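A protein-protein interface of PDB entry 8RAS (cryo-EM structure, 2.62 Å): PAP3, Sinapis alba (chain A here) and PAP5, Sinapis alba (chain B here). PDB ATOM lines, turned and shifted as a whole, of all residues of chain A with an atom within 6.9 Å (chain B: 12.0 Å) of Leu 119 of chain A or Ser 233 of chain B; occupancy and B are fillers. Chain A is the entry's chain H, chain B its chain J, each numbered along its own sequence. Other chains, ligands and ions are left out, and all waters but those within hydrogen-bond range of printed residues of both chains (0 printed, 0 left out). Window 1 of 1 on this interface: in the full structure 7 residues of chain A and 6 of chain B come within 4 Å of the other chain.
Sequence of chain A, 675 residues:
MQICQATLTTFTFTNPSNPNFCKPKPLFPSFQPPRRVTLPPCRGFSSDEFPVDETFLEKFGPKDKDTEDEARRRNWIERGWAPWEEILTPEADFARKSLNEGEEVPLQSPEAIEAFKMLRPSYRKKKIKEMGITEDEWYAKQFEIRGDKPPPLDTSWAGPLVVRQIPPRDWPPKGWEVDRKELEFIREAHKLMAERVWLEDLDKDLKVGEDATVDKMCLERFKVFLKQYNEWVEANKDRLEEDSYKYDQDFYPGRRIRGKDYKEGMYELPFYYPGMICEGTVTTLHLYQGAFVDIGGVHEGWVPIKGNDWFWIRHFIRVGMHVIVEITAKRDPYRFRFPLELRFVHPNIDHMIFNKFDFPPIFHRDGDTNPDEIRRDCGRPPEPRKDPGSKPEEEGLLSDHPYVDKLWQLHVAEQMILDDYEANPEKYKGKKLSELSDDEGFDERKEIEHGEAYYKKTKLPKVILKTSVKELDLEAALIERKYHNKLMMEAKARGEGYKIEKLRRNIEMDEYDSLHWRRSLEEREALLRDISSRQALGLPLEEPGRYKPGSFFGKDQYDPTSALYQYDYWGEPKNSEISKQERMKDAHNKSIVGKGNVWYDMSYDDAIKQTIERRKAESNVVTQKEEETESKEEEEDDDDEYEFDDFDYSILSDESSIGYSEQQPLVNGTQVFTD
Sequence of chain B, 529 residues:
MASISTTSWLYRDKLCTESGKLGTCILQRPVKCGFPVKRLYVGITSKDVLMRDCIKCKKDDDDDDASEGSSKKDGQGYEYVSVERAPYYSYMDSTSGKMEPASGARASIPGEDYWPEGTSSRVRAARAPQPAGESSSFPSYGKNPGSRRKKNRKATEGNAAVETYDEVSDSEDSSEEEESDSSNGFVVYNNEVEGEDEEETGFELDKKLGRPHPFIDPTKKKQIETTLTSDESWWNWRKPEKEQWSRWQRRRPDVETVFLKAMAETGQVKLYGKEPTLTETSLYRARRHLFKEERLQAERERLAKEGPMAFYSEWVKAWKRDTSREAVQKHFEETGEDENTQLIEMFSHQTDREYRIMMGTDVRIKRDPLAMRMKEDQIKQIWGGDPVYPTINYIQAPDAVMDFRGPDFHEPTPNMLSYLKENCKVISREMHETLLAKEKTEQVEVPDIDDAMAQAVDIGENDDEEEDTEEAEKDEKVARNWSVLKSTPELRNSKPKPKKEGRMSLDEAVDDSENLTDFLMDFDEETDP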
ATOM      1  N   PRO A  90      16.847   4.195  29.483  1.00  0.00           N
ATOM      2  CA  PRO A  90      16.817   5.540  30.077  1.00  0.00           C
ATOM      3  C   PRO A  90      15.526   5.842  30.813  1.00  0.00           C
ATOM      4  O   PRO A  90      15.553   6.554  31.824  1.00  0.00           O
ATOM      5  CB  PRO A  90      17.003   6.460  28.864  1.00  0.00           C
ATOM      6  CG  PRO A  90      17.763   5.639  27.894  1.00  0.00           C
ATOM      7  CD  PRO A  90      17.308   4.223  28.083  1.00  0.00           C
ATOM      8  N   GLU A  91      14.396   5.311  30.345  1.00  0.00           N
ATOM      9  CA  GLU A  91      13.124   5.555  31.018  1.00  0.00           C
ATOM     10  C   GLU A  91      13.080   4.882  32.384  1.00  0.00           C
ATOM     11  O   GLU A  91      12.670   5.496  33.374  1.00  0.00           O
ATOM     12  CB  GLU A  91      11.971   5.076  30.138  1.00  0.00           C
ATOM     13  CG  GLU A  91      11.658   5.992  28.973  1.00  0.00           C
ATOM     14  CD  GLU A  91      12.603   5.800  27.806  1.00  0.00           C
ATOM     15  OE1 GLU A  91      13.141   4.685  27.650  1.00  0.00           O
ATOM     16  OE2 GLU A  91      12.811   6.766  27.043  1.00  0.00           O
ATOM     17  N   ALA A  92      13.500   3.616  32.460  1.00  0.00           N
ATOM     18  CA  ALA A  92      13.511   2.917  33.742  1.00  0.00           C
ATOM     19  C   ALA A  92      14.536   3.519  34.694  1.00  0.00           C
ATOM     20  O   ALA A  92      14.282   3.639  35.900  1.00  0.00           O
ATOM     21  CB  ALA A  92      13.786   1.429  33.526  1.00  0.00           C
ATOM     22  N   ASP A  93      15.703   3.900  34.171  1.00  0.00           N
ATOM     23  CA  ASP A  93      16.711   4.556  34.997  1.00  0.00           C
ATOM     24  C   ASP A  93      16.192   5.878  35.550  1.00  0.00           C
ATOM     25  O   ASP A  93      16.401   6.191  36.728  1.00  0.00           O
ATOM     26  CB  ASP A  93      17.986   4.773  34.182  1.00  0.00           C
ATOM     27  CG  ASP A  93      19.145   5.251  35.028  1.00  0.00           C
ATOM     28  OD1 ASP A  93      19.545   4.520  35.958  1.00  0.00           O
ATOM     29  OD2 ASP A  93      19.657   6.356  34.762  1.00  0.00           O
ATOM     30  N   PHE A  94      15.513   6.665  34.712  1.00  0.00           N
ATOM     31  CA  PHE A  94      14.929   7.917  35.178  1.00  0.00           C
ATOM     32  C   PHE A  94      13.838   7.666  36.210  1.00  0.00           C
ATOM     33  O   PHE A  94      13.716   8.412  37.186  1.00  0.00           O
ATOM     34  CB  PHE A  94      14.375   8.711  33.997  1.00  0.00           C
ATOM     35  CG  PHE A  94      13.594   9.928  34.400  1.00  0.00           C
ATOM     36  CD1 PHE A  94      14.215  10.984  35.042  1.00  0.00           C
ATOM     37  CD2 PHE A  94      12.236  10.013  34.143  1.00  0.00           C
ATOM     38  CE1 PHE A  94      13.499  12.101  35.417  1.00  0.00           C
ATOM     39  CE2 PHE A  94      11.515  11.129  34.514  1.00  0.00           C
ATOM     40  CZ  PHE A  94      12.148  12.174  35.153  1.00  0.00           C
ATOM     41  N   ALA A  95      13.029   6.625  36.005  1.00  0.00           N
ATOM     42  CA  ALA A  95      11.981   6.305  36.967  1.00  0.00           C
ATOM     43  C   ALA A  95      12.568   5.931  38.319  1.00  0.00           C
ATOM     44  O   ALA A  95      12.030   6.310  39.364  1.00  0.00           O
ATOM     45  CB  ALA A  95      11.108   5.172  36.431  1.00  0.00           C
ATOM     46  N   GLU A 114      20.606  14.202  35.396  1.00  0.00           N
ATOM     47  CA  GLU A 114      21.222  13.512  34.269  1.00  0.00           C
ATOM     48  C   GLU A 114      20.257  12.514  33.640  1.00  0.00           C
ATOM     49  O   GLU A 114      20.184  12.398  32.411  1.00  0.00           O
ATOM     50  CB  GLU A 114      22.504  12.816  34.723  1.00  0.00           C
ATOM     51  CG  GLU A 114      23.322  12.219  33.593  1.00  0.00           C
ATOM     52  CD  GLU A 114      23.876  13.270  32.656  1.00  0.00           C
ATOM     53  OE1 GLU A 114      24.087  14.418  33.104  1.00  0.00           O
ATOM     54  OE2 GLU A 114      24.101  12.950  31.471  1.00  0.00           O
ATOM     55  N   ALA A 115      19.503  11.787  34.468  1.00  0.00           N
ATOM     56  CA  ALA A 115      18.523  10.841  33.947  1.00  0.00           C
ATOM     57  C   ALA A 115      17.441  11.553  33.146  1.00  0.00           C
ATOM     58  O   ALA A 115      16.989  11.047  32.112  1.00  0.00           O
ATOM     59  CB  ALA A 115      17.908  10.041  35.094  1.00  0.00           C
ATOM     60  N   PHE A 116      17.008  12.725  33.614  1.00  0.00           N
ATOM     61  CA  PHE A 116      16.044  13.521  32.862  1.00  0.00           C
ATOM     62  C   PHE A 116      16.618  13.952  31.519  1.00  0.00           C
ATOM     63  O   PHE A 116      15.917  13.935  30.501  1.00  0.00           O
ATOM     64  CB  PHE A 116      15.625  14.741  33.683  1.00  0.00           C
ATOM     65  CG  PHE A 116      14.398  15.438  33.164  1.00  0.00           C
ATOM     66  CD1 PHE A 116      14.493  16.382  32.155  1.00  0.00           C
ATOM     67  CD2 PHE A 116      13.152  15.160  33.695  1.00  0.00           C
ATOM     68  CE1 PHE A 116      13.368  17.024  31.681  1.00  0.00           C
ATOM     69  CE2 PHE A 116      12.024  15.800  33.225  1.00  0.00           C
ATOM     70  CZ  PHE A 116      12.132  16.733  32.217  1.00  0.00           C
ATOM     71  N   LYS A 117      17.891  14.349  31.498  1.00  0.00           N
ATOM     72  CA  LYS A 117      18.515  14.778  30.251  1.00  0.00           C
ATOM     73  C   LYS A 117      18.680  13.623  29.273  1.00  0.00           C
ATOM     74  O   LYS A 117      18.574  13.824  28.058  1.00  0.00           O
ATOM     75  CB  LYS A 117      19.869  15.424  30.540  1.00  0.00           C
ATOM     76  CG  LYS A 117      19.786  16.735  31.302  1.00  0.00           C
ATOM     77  CD  LYS A 117      19.427  17.889  30.384  1.00  0.00           C
ATOM     78  CE  LYS A 117      19.148  19.154  31.177  1.00  0.00           C
ATOM     79  NZ  LYS A 117      20.350  19.614  31.926  1.00  0.00           N
ATOM     80  N   MET A 118      18.933  12.416  29.773  1.00  0.00           N
ATOM     81  CA  MET A 118      19.153  11.254  28.922  1.00  0.00           C
ATOM     82  C   MET A 118      17.867  10.686  28.337  1.00  0.00           C
ATOM     83  O   MET A 118      17.936   9.748  27.537  1.00  0.00           O
ATOM     84  CB  MET A 118      19.889  10.161  29.701  1.00  0.00           C
ATOM     85  CG  MET A 118      21.298  10.538  30.122  1.00  0.00           C
ATOM     86  SD  MET A 118      22.442  10.605  28.733  1.00  0.00           S
ATOM     87  CE  MET A 118      22.805   8.866  28.517  1.00  0.00           C
ATOM     88  N   LEU A 119      16.705  11.219  28.719  1.00  0.00           N
ATOM     89  CA  LEU A 119      15.446  10.753  28.150  1.00  0.00           C
ATOM     90  C   LEU A 119      15.360  11.007  26.651  1.00  0.00           C
ATOM     91  O   LEU A 119      14.599  10.323  25.960  1.00  0.00           O
ATOM     92  CB  LEU A 119      14.270  11.424  28.859  1.00  0.00           C
ATOM     93  CG  LEU A 119      14.075  11.057  30.329  1.00  0.00           C
ATOM     94  CD1 LEU A 119      12.999  11.925  30.956  1.00  0.00           C
ATOM     95  CD2 LEU A 119      13.730   9.587  30.468  1.00  0.00           C
ATOM     96  N   ARG A 120      16.117  11.975  26.135  1.00  0.00           N
ATOM     97  CA  ARG A 120      16.148  12.244  24.707  1.00  0.00           C
ATOM     98  C   ARG A 120      17.393  11.620  24.103  1.00  0.00           C
ATOM     99  O   ARG A 120      18.510  11.984  24.504  1.00  0.00           O
ATOM    100  CB  ARG A 120      16.131  13.745  24.445  1.00  0.00           C
ATOM    101  CG  ARG A 120      14.902  14.451  24.985  1.00  0.00           C
ATOM    102  CD  ARG A 120      14.987  15.949  24.764  1.00  0.00           C
ATOM    103  NE  ARG A 120      13.820  16.645  25.292  1.00  0.00           N
ATOM    104  CZ  ARG A 120      13.825  17.902  25.710  1.00  0.00           C
ATOM    105  NH1 ARG A 120      14.923  18.639  25.675  1.00  0.00           N
ATOM    106  NH2 ARG A 120      12.700  18.435  26.177  1.00  0.00           N
ATOM    107  N   PRO A 121      17.262  10.682  23.163  1.00  0.00           N
ATOM    108  CA  PRO A 121      18.460  10.075  22.560  1.00  0.00           C
ATOM    109  C   PRO A 121      19.355  11.066  21.837  1.00  0.00           C
ATOM    110  O   PRO A 121      20.543  10.779  21.655  1.00  0.00           O
ATOM    111  CB  PRO A 121      17.887   9.028  21.592  1.00  0.00           C
ATOM    112  CG  PRO A 121      16.417   9.273  21.529  1.00  0.00           C
ATOM    113  CD  PRO A 121      16.023   9.995  22.768  1.00  0.00           C
ATOM    114  N   SER A 122      18.827  12.215  21.405  1.00  0.00           N
ATOM    115  CA  SER A 122      19.676  13.229  20.786  1.00  0.00           C
ATOM    116  C   SER A 122      20.696  13.773  21.778  1.00  0.00           C
ATOM    117  O   SER A 122      21.869  13.971  21.433  1.00  0.00           O
ATOM    118  CB  SER A 122      18.816  14.359  20.224  1.00  0.00           C
ATOM    119  OG  SER A 122      18.192  15.085  21.267  1.00  0.00           O
ATOM    120  N   TYR A 123      20.269  14.023  23.019  1.00  0.00           N
ATOM    121  CA  TYR A 123      21.207  14.455  24.048  1.00  0.00           C
ATOM    122  C   TYR A 123      22.246  13.378  24.324  1.00  0.00           C
ATOM    123  O   TYR A 123      23.425  13.682  24.540  1.00  0.00           O
ATOM    124  CB  TYR A 123      20.460  14.814  25.331  1.00  0.00           C
ATOM    125  CG  TYR A 123      21.373  15.091  26.507  1.00  0.00           C
ATOM    126  CD1 TYR A 123      21.960  16.336  26.677  1.00  0.00           C
ATOM    127  CD2 TYR A 123      21.649  14.104  27.445  1.00  0.00           C
ATOM    128  CE1 TYR A 123      22.794  16.593  27.748  1.00  0.00           C
ATOM    129  CE2 TYR A 123      22.483  14.351  28.517  1.00  0.00           C
ATOM    130  CZ  TYR A 123      23.051  15.597  28.664  1.00  0.00           C
ATOM    131  OH  TYR A 123      23.882  15.848  29.732  1.00  0.00           O
ATOM    132  N   ARG A 124      21.823  12.114  24.336  1.00  0.00           N
ATOM    133  CA  ARG A 124      22.765  11.022  24.548  1.00  0.00           C
ATOM    134  C   ARG A 124      23.797  10.963  23.430  1.00  0.00           C
ATOM    135  O   ARG A 124      24.987  10.762  23.687  1.00  0.00           O
ATOM    136  CB  ARG A 124      22.011   9.697  24.662  1.00  0.00           C
ATOM    137  CG  ARG A 124      22.757   8.505  24.092  1.00  0.00           C
ATOM    138  CD  ARG A 124      22.282   7.209  24.719  1.00  0.00           C
ATOM    139  NE  ARG A 124      20.839   7.027  24.616  1.00  0.00           N
ATOM    140  CZ  ARG A 124      20.205   6.665  23.509  1.00  0.00           C
ATOM    141  NH1 ARG A 124      20.856   6.447  22.378  1.00  0.00           N
ATOM    142  NH2 ARG A 124      18.885   6.511  23.539  1.00  0.00           N
ATOM    143  N   THR B 226      10.276  22.800  11.153  1.00  0.00           N
ATOM    144  CA  THR B 226      10.547  21.408  11.478  1.00  0.00           C
ATOM    145  C   THR B 226      10.453  21.228  12.986  1.00  0.00           C
ATOM    146  O   THR B 226      11.017  22.021  13.746  1.00  0.00           O
ATOM    147  CB  THR B 226      11.930  20.979  10.979  1.00  0.00           C
ATOM    148  OG1 THR B 226      12.109  21.417   9.627  1.00  0.00           O
ATOM    149  CG2 THR B 226      12.072  19.467  11.037  1.00  0.00           C
ATOM    150  N   THR B 227       9.742  20.192  13.413  1.00  0.00           N
ATOM    151  CA  THR B 227       9.516  19.911  14.820  1.00  0.00           C
ATOM    152  C   THR B 227      10.362  18.715  15.251  1.00  0.00           C
ATOM    153  O   THR B 227      11.197  18.211  14.491  1.00  0.00           O
ATOM    154  CB  THR B 227       8.026  19.681  15.074  1.00  0.00           C
ATOM    155  OG1 THR B 227       7.511  18.761  14.105  1.00  0.00           O
ATOM    156  CG2 THR B 227       7.266  20.993  14.969  1.00  0.00           C
ATOM    157  N   LEU B 228      10.148  18.267  16.487  1.00  0.00           N
ATOM    158  CA  LEU B 228      10.920  17.159  17.034  1.00  0.00           C
ATOM    159  C   LEU B 228      10.746  15.908  16.182  1.00  0.00           C
ATOM    160  O   LEU B 228       9.641  15.590  15.732  1.00  0.00           O
ATOM    161  CB  LEU B 228      10.496  16.882  18.476  1.00  0.00           C
ATOM    162  CG  LEU B 228      10.577  18.062  19.447  1.00  0.00           C
ATOM    163  CD1 LEU B 228      10.287  17.610  20.866  1.00  0.00           C
ATOM    164  CD2 LEU B 228      11.930  18.742  19.367  1.00  0.00           C
ATOM    165  N   THR B 229      11.850  15.196  15.959  1.00  0.00           N
ATOM    166  CA  THR B 229      11.888  14.047  15.061  1.00  0.00           C
ATOM    167  C   THR B 229      11.890  12.718  15.808  1.00  0.00           C
ATOM    168  O   THR B 229      12.405  11.721  15.292  1.00  0.00           O
ATOM    169  CB  THR B 229      13.106  14.134  14.143  1.00  0.00           C
ATOM    170  OG1 THR B 229      14.228  13.509  14.777  1.00  0.00           O
ATOM    171  CG2 THR B 229      13.444  15.585  13.838  1.00  0.00           C
ATOM    172  N   SER B 230      11.345  12.693  17.025  1.00  0.00           N
ATOM    173  CA  SER B 230      11.227  11.525  17.895  1.00  0.00           C
ATOM    174  C   SER B 230      12.573  11.042  18.416  1.00  0.00           C
ATOM    175  O   SER B 230      12.606  10.120  19.239  1.00  0.00           O
ATOM    176  CB  SER B 230      10.507  10.350  17.215  1.00  0.00           C
ATOM    177  OG  SER B 230      10.654   9.159  17.967  1.00  0.00           O
ATOM    178  N   ASP B 231      13.683  11.629  17.972  1.00  0.00           N
ATOM    179  CA  ASP B 231      14.989  11.363  18.552  1.00  0.00           C
ATOM    180  C   ASP B 231      15.401  12.424  19.560  1.00  0.00           C
ATOM    181  O   ASP B 231      16.343  12.201  20.326  1.00  0.00           O
ATOM    182  CB  ASP B 231      16.052  11.270  17.451  1.00  0.00           C
ATOM    183  CG  ASP B 231      17.008  10.115  17.662  1.00  0.00           C
ATOM    184  OD1 ASP B 231      16.588   9.095  18.248  1.00  0.00           O
ATOM    185  OD2 ASP B 231      18.177  10.226  17.243  1.00  0.00           O
ATOM    186  N   GLU B 232      14.721  13.569  19.563  1.00  0.00           N
ATOM    187  CA  GLU B 232      14.916  14.617  20.555  1.00  0.00           C
ATOM    188  C   GLU B 232      13.640  14.845  21.356  1.00  0.00           C
ATOM    189  O   GLU B 232      13.369  15.957  21.811  1.00  0.00           O
ATOM    190  CB  GLU B 232      15.375  15.912  19.887  1.00  0.00           C
ATOM    191  CG  GLU B 232      14.529  16.330  18.700  1.00  0.00           C
ATOM    192  CD  GLU B 232      15.180  15.998  17.373  1.00  0.00           C
ATOM    193  OE1 GLU B 232      15.823  14.932  17.275  1.00  0.00           O
ATOM    194  OE2 GLU B 232      15.051  16.806  16.431  1.00  0.00           O
ATOM    195  N   SER B 233      12.849  13.790  21.532  1.00  0.00           N
ATOM    196  CA  SER B 233      11.563  13.875  22.204  1.00  0.00           C
ATOM    197  C   SER B 233      11.493  12.844  23.320  1.00  0.00           C
ATOM    198  O   SER B 233      12.155  11.805  23.271  1.00  0.00           O
ATOM    199  CB  SER B 233      10.405  13.652  21.223  1.00  0.00           C
ATOM    200  OG  SER B 233       9.158  13.690  21.892  1.00  0.00           O
ATOM    201  N   TRP B 234      10.684  13.147  24.330  1.00  0.00           N
ATOM    202  CA  TRP B 234      10.434  12.198  25.400  1.00  0.00           C
ATOM    203  C   TRP B 234       9.573  11.045  24.894  1.00  0.00           C
ATOM    204  O   TRP B 234       8.943  11.120  23.836  1.00  0.00           O
ATOM    205  CB  TRP B 234       9.756  12.886  26.582  1.00  0.00           C
ATOM    206  CG  TRP B 234      10.575  13.978  27.191  1.00  0.00           C
ATOM    207  CD1 TRP B 234      11.934  14.044  27.256  1.00  0.00           C
ATOM    208  CD2 TRP B 234      10.085  15.165  27.825  1.00  0.00           C
ATOM    209  NE1 TRP B 234      12.323  15.197  27.891  1.00  0.00           N
ATOM    210  CE2 TRP B 234      11.205  15.904  28.249  1.00  0.00           C
ATOM    211  CE3 TRP B 234       8.807  15.675  28.074  1.00  0.00           C
ATOM    212  CZ2 TRP B 234      11.088  17.124  28.908  1.00  0.00           C
ATOM    213  CZ3 TRP B 234       8.693  16.887  28.729  1.00  0.00           C
ATOM    214  CH2 TRP B 234       9.826  17.598  29.138  1.00  0.00           C
ATOM    215  N   TRP B 235       9.553   9.961  25.671  1.00  0.00           N
ATOM    216  CA  TRP B 235       8.852   8.755  25.245  1.00  0.00           C
ATOM    217  C   TRP B 235       7.354   8.998  25.102  1.00  0.00           C
ATOM    218  O   TRP B 235       6.715   8.459  24.192  1.00  0.00           O
ATOM    219  CB  TRP B 235       9.120   7.617  26.230  1.00  0.00           C
ATOM    220  CG  TRP B 235       8.681   7.910  27.630  1.00  0.00           C
ATOM    221  CD1 TRP B 235       9.403   8.539  28.601  1.00  0.00           C
ATOM    222  CD2 TRP B 235       7.417   7.584  28.219  1.00  0.00           C
ATOM    223  NE1 TRP B 235       8.668   8.624  29.757  1.00  0.00           N
ATOM    224  CE2 TRP B 235       7.444   8.047  29.548  1.00  0.00           C
ATOM    225  CE3 TRP B 235       6.264   6.950  27.750  1.00  0.00           C
ATOM    226  CZ2 TRP B 235       6.366   7.891  30.412  1.00  0.00           C
ATOM    227  CZ3 TRP B 235       5.196   6.798  28.610  1.00  0.00           C
ATOM    228  CH2 TRP B 235       5.253   7.265  29.925  1.00  0.00           C
ATOM    229  N   ASN B 236       6.776   9.807  25.990  1.00  0.00           N
ATOM    230  CA  ASN B 236       5.335  10.030  25.979  1.00  0.00           C
ATOM    231  C   ASN B 236       4.878  10.937  24.845  1.00  0.00           C
ATOM    232  O   ASN B 236       3.670  11.038  24.610  1.00  0.00           O
ATOM    233  CB  ASN B 236       4.887  10.613  27.321  1.00  0.00           C
ATOM    234  CG  ASN B 236       5.706  11.816  27.735  1.00  0.00           C
ATOM    235  OD1 ASN B 236       6.932  11.795  27.677  1.00  0.00           O
ATOM    236  ND2 ASN B 236       5.027  12.876  28.156  1.00  0.00           N
ATOM    237  N   TRP B 237       5.799  11.594  24.140  1.00  0.00           N
ATOM    238  CA  TRP B 237       5.455  12.482  23.038  1.00  0.00           C
ATOM    239  C   TRP B 237       5.934  11.951  21.692  1.00  0.00           C
ATOM    240  O   TRP B 237       6.073  12.723  20.739  1.00  0.00           O
ATOM    241  CB  TRP B 237       6.021  13.881  23.283  1.00  0.00           C
ATOM    242  CG  TRP B 237       5.322  14.651  24.367  1.00  0.00           C
ATOM    243  CD1 TRP B 237       5.906  15.268  25.432  1.00  0.00           C
ATOM    244  CD2 TRP B 237       3.913  14.896  24.485  1.00  0.00           C
ATOM    245  NE1 TRP B 237       4.952  15.875  26.210  1.00  0.00           N
ATOM    246  CE2 TRP B 237       3.721  15.663  25.650  1.00  0.00           C
ATOM    247  CE3 TRP B 237       2.797  14.541  23.721  1.00  0.00           C
ATOM    248  CZ2 TRP B 237       2.460  16.079  26.069  1.00  0.00           C
ATOM    249  CZ3 TRP B 237       1.548  14.953  24.140  1.00  0.00           C
ATOM    250  CH2 TRP B 237       1.389  15.715  25.302  1.00  0.00           C
ATOM    251  N   ARG B 238       6.191  10.651  21.593  1.00  0.00           N
ATOM    252  CA  ARG B 238       6.680  10.042  20.364  1.00  0.00           C
ATOM    253  C   ARG B 238       5.526   9.454  19.564  1.00  0.00           C
ATOM    254  O   ARG B 238       4.627   8.819  20.122  1.00  0.00           O
ATOM    255  CB  ARG B 238       7.708   8.949  20.663  1.00  0.00           C
ATOM    256  CG  ARG B 238       9.080   9.472  21.030  1.00  0.00           C
ATOM    257  CD  ARG B 238      10.012   8.336  21.401  1.00  0.00           C
ATOM    258  NE  ARG B 238      11.240   8.822  22.019  1.00  0.00           N
ATOM    259  CZ  ARG B 238      11.917   8.167  22.952  1.00  0.00           C
ATOM    260  NH1 ARG B 238      11.516   6.990  23.398  1.00  0.00           N
ATOM    261  NH2 ARG B 238      13.022   8.710  23.450  1.00  0.00           N
ATOM    262  N   LYS B 239       5.558   9.677  18.258  1.00  0.00           N
ATOM    263  CA  LYS B 239       4.551   9.113  17.372  1.00  0.00           C
ATOM    264  C   LYS B 239       4.762   7.601  17.312  1.00  0.00           C
ATOM    265  O   LYS B 239       5.880   7.150  17.040  1.00  0.00           O
ATOM    266  CB  LYS B 239       4.676   9.775  15.989  1.00  0.00           C
ATOM    267  CG  LYS B 239       3.573   9.555  14.922  1.00  0.00           C
ATOM    268  CD  LYS B 239       3.154   8.122  14.660  1.00  0.00           C
ATOM    269  CE  LYS B 239       1.941   8.047  13.746  1.00  0.00           C
ATOM    270  NZ  LYS B 239       1.338   6.684  13.728  1.00  0.00           N
ATOM    271  N   PRO B 240       3.732   6.795  17.581  1.00  0.00           N
ATOM    272  CA  PRO B 240       3.919   5.338  17.602  1.00  0.00           C
ATOM    273  C   PRO B 240       4.415   4.802  16.267  1.00  0.00           C
ATOM    274  O   PRO B 240       4.059   5.301  15.199  1.00  0.00           O
ATOM    275  CB  PRO B 240       2.519   4.807  17.929  1.00  0.00           C
ATOM    276  CG  PRO B 240       1.851   5.927  18.649  1.00  0.00           C
ATOM    277  CD  PRO B 240       2.394   7.192  18.051  1.00  0.00           C
ATOM    278  N   GLU B 241       5.250   3.764  16.344  1.00  0.00           N
ATOM    279  CA  GLU B 241       5.856   3.207  15.136  1.00  0.00           C
ATOM    280  C   GLU B 241       4.797   2.689  14.171  1.00  0.00           C
ATOM    281  O   GLU B 241       4.896   2.905  12.957  1.00  0.00           O
ATOM    282  CB  GLU B 241       6.836   2.092  15.507  1.00  0.00           C
ATOM    283  CG  GLU B 241       7.838   2.457  16.599  1.00  0.00           C
ATOM    284  CD  GLU B 241       7.294   2.247  18.001  1.00  0.00           C
ATOM    285  OE1 GLU B 241       6.075   2.012  18.142  1.00  0.00           O
ATOM    286  OE2 GLU B 241       8.086   2.318  18.964  1.00  0.00           O
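NE1 of Trp 234 of chain B sits close to NE of Arg 120 of chain A (3.3 Å).
N of Ser 122 of chain A is in hydrogen-bond range of O of Asp 231 of chain B (2.7 Å).
The guanidinium group (NH1) of Arg 238 of chain B lies within salt-bridge range of the side-chain carboxylate (OE2) of Glu 91 of chain A (3.9 Å).
The backbone carbonyl oxygen of Asp 231 of chain B lies close to the backbone nitrogen of Pro 121 of chain A (3.3 Å).
The backbone carbonyl oxygen (O) of Leu 119 of chain A lies within hydrogen-bond range of the guanidinium group (NH2) of Arg 238 of chain B, 3.4 Å away.
The side-chain hydroxyl (OG1) of Thr 229 of chain B is in hydrogen-bond range of the side-chain carboxylate (OE1) of Glu 232 of chain B, 3.3 Å away.
O of Ser 230 of chain B lies within hydrogen-bond range of NE of Arg 238 of chain B (3.4 Å).
The guanidinium group of Arg 238 of chain B lies within hydrogen-bond range of the backbone carbonyl oxygen of Ser 233 of chain B (3.2 Å).
CD1 of Trp 235 of chain B touches CG of Glu 91 of chain A, at 3.4 Å.
Phe 116 of chain A touches Trp 234 of chain B (CZ to CZ2, 3.5 Å).
Ser 233 of chain B touches Leu 119 of chain A (O to O, 3.9 Å).
CD1 of Trp 234 of chain B touches CB of Leu 119 of chain A, 3.9 Å away.
CD of Arg 120 of chain A touches O of Glu 232 of chain B, 3.4 Å away.
Arg 238 of chain B touches Pro 121 of chain A.
CB of Glu 232 of chain B touches OG of Ser 122 of chain A, 3.2 Å away.
Of chain B, only Trp 235 (3.4 Å) and Arg 238 (3.9 Å) come within 4 Å of Glu 91 of chain A.
Of chain B, only Trp 234 comes within 4 Å of Phe 116 of chain A.
No residue of chain B comes within 4 Å of Met 118 of chain A.
Arg 120 of chain A touches three residues of chain B.
Of chain B, only Asp 231 and Arg 238 come within 4 Å of Pro 121 of chain A.
Of the printed residues of chain A, Asp 231 of chain B touches Arg 120 (3.96 Å), Pro 121 (3.2 Å) and Ser 122 (2.7 Å).
Printed residues of chain A within 4 Å of Trp 234 of chain B: Phe 116 (3.5 Å), Leu 119 (3.9 Å) and Arg 120 (3.3 Å).
Of the printed residues of chain B, Ser 122 of chain A touches Asp 231 and Glu 232.
The nearest residue of chain A that does not touch Ser 233 of chain B is Arg 120 of chain A (4.1 Å).
Of the 16 printed residues of chain B, 6 touch a printed residue of chain A.
Among the printed residues, 13 pairs touch across the chains.
Among the printed residues, Asp or Glu carboxylates within 4 Å of a Lys or Arg side-chain nitrogen of the other chain: Glu 91 of chain A with Arg 238 of chain B (3.9 Å).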
